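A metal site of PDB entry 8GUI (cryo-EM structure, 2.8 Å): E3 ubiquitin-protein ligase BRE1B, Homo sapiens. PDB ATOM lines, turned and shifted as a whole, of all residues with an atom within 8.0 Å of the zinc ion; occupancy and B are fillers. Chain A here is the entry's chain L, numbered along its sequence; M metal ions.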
ATOM      1  N   LEU A 960      23.472  22.031  12.526  1.00  0.00           N
ATOM      2  CA  LEU A 960      22.150  22.637  12.608  1.00  0.00           C
ATOM      3  C   LEU A 960      21.100  21.533  12.590  1.00  0.00           C
ATOM      4  O   LEU A 960      21.051  20.739  11.646  1.00  0.00           O
ATOM      5  CB  LEU A 960      21.920  23.617  11.456  1.00  0.00           C
ATOM      6  CG  LEU A 960      22.778  24.884  11.433  1.00  0.00           C
ATOM      7  CD1 LEU A 960      22.528  25.669  10.162  1.00  0.00           C
ATOM      8  CD2 LEU A 960      22.501  25.729  12.658  1.00  0.00           C
ATOM      9  N   LYS A 962      17.935  21.536  12.159  1.00  0.00           N
ATOM     10  CA  LYS A 962      16.798  21.679  11.259  1.00  0.00           C
ATOM     11  C   LYS A 962      17.195  21.628   9.786  1.00  0.00           C
ATOM     12  O   LYS A 962      16.325  21.755   8.917  1.00  0.00           O
ATOM     13  CB  LYS A 962      16.039  22.976  11.541  1.00  0.00           C
ATOM     14  CG  LYS A 962      15.070  22.927  12.730  1.00  0.00           C
ATOM     15  CD  LYS A 962      15.780  22.909  14.078  1.00  0.00           C
ATOM     16  CE  LYS A 962      14.775  22.945  15.222  1.00  0.00           C
ATOM     17  NZ  LYS A 962      15.437  22.813  16.550  1.00  0.00           N
ATOM     18  N   CYS A 963      18.473  21.447   9.482  1.00  0.00           N
ATOM     19  CA  CYS A 963      18.918  21.291   8.099  1.00  0.00           C
ATOM     20  C   CYS A 963      19.960  20.199   7.913  1.00  0.00           C
ATOM     21  O   CYS A 963      20.370  19.972   6.765  1.00  0.00           O
ATOM     22  CB  CYS A 963      19.488  22.614   7.562  1.00  0.00           C
ATOM     23  SG  CYS A 963      21.196  22.923   8.015  1.00  0.00           S
ATOM     24  N   PHE A 964      20.388  19.531   8.986  1.00  0.00           N
ATOM     25  CA  PHE A 964      21.223  18.330   8.904  1.00  0.00           C
ATOM     26  C   PHE A 964      22.578  18.611   8.244  1.00  0.00           C
ATOM     27  O   PHE A 964      23.119  17.784   7.516  1.00  0.00           O
ATOM     28  CB  PHE A 964      20.487  17.203   8.170  1.00  0.00           C
ATOM     29  CG  PHE A 964      19.596  16.377   9.055  1.00  0.00           C
ATOM     30  CD1 PHE A 964      19.155  16.858  10.276  1.00  0.00           C
ATOM     31  CD2 PHE A 964      19.178  15.127   8.645  1.00  0.00           C
ATOM     32  CE1 PHE A 964      18.323  16.112  11.073  1.00  0.00           C
ATOM     33  CE2 PHE A 964      18.341  14.358   9.442  1.00  0.00           C
ATOM     34  CZ  PHE A 964      17.917  14.856  10.659  1.00  0.00           C
ATOM     35  N   HIS A 965      23.135  19.797   8.502  1.00  0.00           N
ATOM     36  CA  HIS A 965      24.403  20.198   7.930  1.00  0.00           C
ATOM     37  C   HIS A 965      25.388  20.543   9.040  1.00  0.00           C
ATOM     38  O   HIS A 965      25.006  21.008  10.114  1.00  0.00           O
ATOM     39  CB  HIS A 965      24.245  21.400   6.996  1.00  0.00           C
ATOM     40  CG  HIS A 965      23.298  21.176   5.867  1.00  0.00           C
ATOM     41  ND1 HIS A 965      22.266  22.039   5.568  1.00  0.00           N
ATOM     42  CD2 HIS A 965      23.227  20.176   4.955  1.00  0.00           C
ATOM     43  CE1 HIS A 965      21.594  21.590   4.521  1.00  0.00           C
ATOM     44  NE2 HIS A 965      22.152  20.455   4.131  1.00  0.00           N
ATOM     45  N   VAL A 966      26.674  20.314   8.767  1.00  0.00           N
ATOM     46  CA  VAL A 966      27.729  20.477   9.748  1.00  0.00           C
ATOM     47  C   VAL A 966      28.406  21.824   9.519  1.00  0.00           C
ATOM     48  O   VAL A 966      28.823  22.136   8.394  1.00  0.00           O
ATOM     49  CB  VAL A 966      28.756  19.341   9.663  1.00  0.00           C
ATOM     50  CG1 VAL A 966      29.688  19.362  10.871  1.00  0.00           C
ATOM     51  CG2 VAL A 966      28.059  18.009   9.520  1.00  0.00           C
ATOM     52  N   PHE A 967      28.509  22.629  10.577  1.00  0.00           N
ATOM     53  CA  PHE A 967      29.192  23.912  10.517  1.00  0.00           C
ATOM     54  C   PHE A 967      30.144  24.047  11.691  1.00  0.00           C
ATOM     55  O   PHE A 967      30.351  23.096  12.445  1.00  0.00           O
ATOM     56  CB  PHE A 967      28.176  25.060  10.517  1.00  0.00           C
ATOM     57  CG  PHE A 967      27.457  25.222   9.219  1.00  0.00           C
ATOM     58  CD1 PHE A 967      28.128  25.127   8.010  1.00  0.00           C
ATOM     59  CD2 PHE A 967      26.087  25.459   9.199  1.00  0.00           C
ATOM     60  CE1 PHE A 967      27.458  25.280   6.817  1.00  0.00           C
ATOM     61  CE2 PHE A 967      25.418  25.603   8.001  1.00  0.00           C
ATOM     62  CZ  PHE A 967      26.109  25.516   6.806  1.00  0.00           C
ATOM     63  N   LYS A 982      19.578  32.482   8.965  1.00  0.00           N
ATOM     64  CA  LYS A 982      19.610  31.809   7.684  1.00  0.00           C
ATOM     65  C   LYS A 982      20.793  30.853   7.670  1.00  0.00           C
ATOM     66  O   LYS A 982      21.900  31.224   8.068  1.00  0.00           O
ATOM     67  CB  LYS A 982      19.733  32.811   6.521  1.00  0.00           C
ATOM     68  CG  LYS A 982      18.594  33.831   6.363  1.00  0.00           C
ATOM     69  CD  LYS A 982      17.295  33.214   5.831  1.00  0.00           C
ATOM     70  CE  LYS A 982      16.301  32.832   6.922  1.00  0.00           C
ATOM     71  NZ  LYS A 982      15.009  32.339   6.374  1.00  0.00           N
ATOM     72  N   CYS A 983      20.555  29.624   7.225  1.00  0.00           N
ATOM     73  CA  CYS A 983      21.642  28.654   7.131  1.00  0.00           C
ATOM     74  C   CYS A 983      22.611  29.063   6.021  1.00  0.00           C
ATOM     75  O   CYS A 983      22.186  29.454   4.933  1.00  0.00           O
ATOM     76  CB  CYS A 983      21.095  27.256   6.867  1.00  0.00           C
ATOM     77  SG  CYS A 983      22.369  26.064   6.415  1.00  0.00           S
ATOM     78  N   PRO A 984      23.920  28.991   6.274  1.00  0.00           N
ATOM     79  CA  PRO A 984      24.879  29.238   5.185  1.00  0.00           C
ATOM     80  C   PRO A 984      24.760  28.267   4.022  1.00  0.00           C
ATOM     81  O   PRO A 984      25.129  28.614   2.896  1.00  0.00           O
ATOM     82  CB  PRO A 984      26.235  29.101   5.895  1.00  0.00           C
ATOM     83  CG  PRO A 984      25.962  29.417   7.326  1.00  0.00           C
ATOM     84  CD  PRO A 984      24.569  28.929   7.593  1.00  0.00           C
ATOM     85  N   LYS A 985      24.251  27.052   4.262  1.00  0.00           N
ATOM     86  CA  LYS A 985      24.144  26.051   3.207  1.00  0.00           C
ATOM     87  C   LYS A 985      22.779  26.068   2.526  1.00  0.00           C
ATOM     88  O   LYS A 985      22.679  26.280   1.317  1.00  0.00           O
ATOM     89  CB  LYS A 985      24.442  24.663   3.781  1.00  0.00           C
ATOM     90  CG  LYS A 985      24.369  23.536   2.761  1.00  0.00           C
ATOM     91  CD  LYS A 985      25.582  23.540   1.848  1.00  0.00           C
ATOM     92  CE  LYS A 985      25.569  22.343   0.923  1.00  0.00           C
ATOM     93  NZ  LYS A 985      25.677  21.063   1.675  1.00  0.00           N
ATOM     94  N   CYS A 986      21.707  25.837   3.294  1.00  0.00           N
ATOM     95  CA  CYS A 986      20.374  25.659   2.738  1.00  0.00           C
ATOM     96  C   CYS A 986      19.412  26.775   3.133  1.00  0.00           C
ATOM     97  O   CYS A 986      18.219  26.674   2.842  1.00  0.00           O
ATOM     98  CB  CYS A 986      19.806  24.301   3.145  1.00  0.00           C
ATOM     99  SG  CYS A 986      19.449  24.145   4.904  1.00  0.00           S
ATOM    100  N   ASN A 987      19.891  27.817   3.816  1.00  0.00           N
ATOM    101  CA  ASN A 987      19.102  28.990   4.195  1.00  0.00           C
ATOM    102  C   ASN A 987      17.906  28.638   5.079  1.00  0.00           C
ATOM    103  O   ASN A 987      16.948  29.419   5.171  1.00  0.00           O
ATOM    104  CB  ASN A 987      18.637  29.774   2.970  1.00  0.00           C
ATOM    105  CG  ASN A 987      19.791  30.235   2.100  1.00  0.00           C
ATOM    106  OD1 ASN A 987      20.292  29.478   1.263  1.00  0.00           O
ATOM    107  ND2 ASN A 987      20.229  31.476   2.292  1.00  0.00           N
ATOM    108  N   ALA A 988      17.940  27.491   5.745  1.00  0.00           N
ATOM    109  CA  ALA A 988      16.851  27.110   6.640  1.00  0.00           C
ATOM    110  C   ALA A 988      16.912  27.942   7.916  1.00  0.00           C
ATOM    111  O   ALA A 988      17.985  28.256   8.434  1.00  0.00           O
ATOM    112  CB  ALA A 988      16.922  25.624   6.978  1.00  0.00           C
ATOM    113  N   ALA A 989      15.735  28.301   8.427  1.00  0.00           N
ATOM    114  CA  ALA A 989      15.656  29.070   9.658  1.00  0.00           C
ATOM    115  C   ALA A 989      16.043  28.216  10.853  1.00  0.00           C
ATOM    116  O   ALA A 989      15.718  27.033  10.929  1.00  0.00           O
ATOM    117  CB  ALA A 989      14.246  29.636   9.849  1.00  0.00           C
ATOM    118  N   PHE A 990      16.768  28.831  11.800  1.00  0.00           N
ATOM    119  CA  PHE A 990      17.174  28.145  13.010  1.00  0.00           C
ATOM    120  C   PHE A 990      17.325  29.168  14.130  1.00  0.00           C
ATOM    121  O   PHE A 990      17.480  30.369  13.883  1.00  0.00           O
ATOM    122  CB  PHE A 990      18.465  27.347  12.822  1.00  0.00           C
ATOM    123  CG  PHE A 990      19.643  28.185  12.408  1.00  0.00           C
ATOM    124  CD1 PHE A 990      19.850  28.511  11.080  1.00  0.00           C
ATOM    125  CD2 PHE A 990      20.552  28.635  13.350  1.00  0.00           C
ATOM    126  CE1 PHE A 990      20.938  29.282  10.693  1.00  0.00           C
ATOM    127  CE2 PHE A 990      21.639  29.410  12.978  1.00  0.00           C
ATOM    128  CZ  PHE A 990      21.829  29.724  11.644  1.00  0.00           C
HETATM  129 ZN    ZN M   1      21.517  23.957   5.959  1.00  0.00          ZN
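The backbone carbonyl oxygen (O) of His 965 sits at hydrogen-bond distance from the backbone NH (N) of Leu 960 (3.0 Å). The backbone NH (N) of Lys 985 sits close to the side-chain sulfur (SG) of Cys 983 (3.0 Å). The backbone carbonyl oxygen (O) of Ala 988 is in hydrogen-bond range of the backbone NH (N) of Cys 983 (3.2 Å). The side-chain sulfur (SG) of Cys 986 lies close to the backbone NH (N) of Ala 988, 3.8 Å away.
Lys 985 touches the zinc ion (CB to ZN, 3.7 Å). Of the 16 residues printed, 5 come within 4 Å of the zinc ion.
The zinc ion is bound by a ring nitrogen (ND1) of His 965. The zinc ion is bound by the side-chain sulfur (SG) of Cys 983 (2.3 Å). The zinc ion is bound by SG of Cys 963 (2.3 Å). SG of Cys 986 binds the zinc ion, at 2.3 Å.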
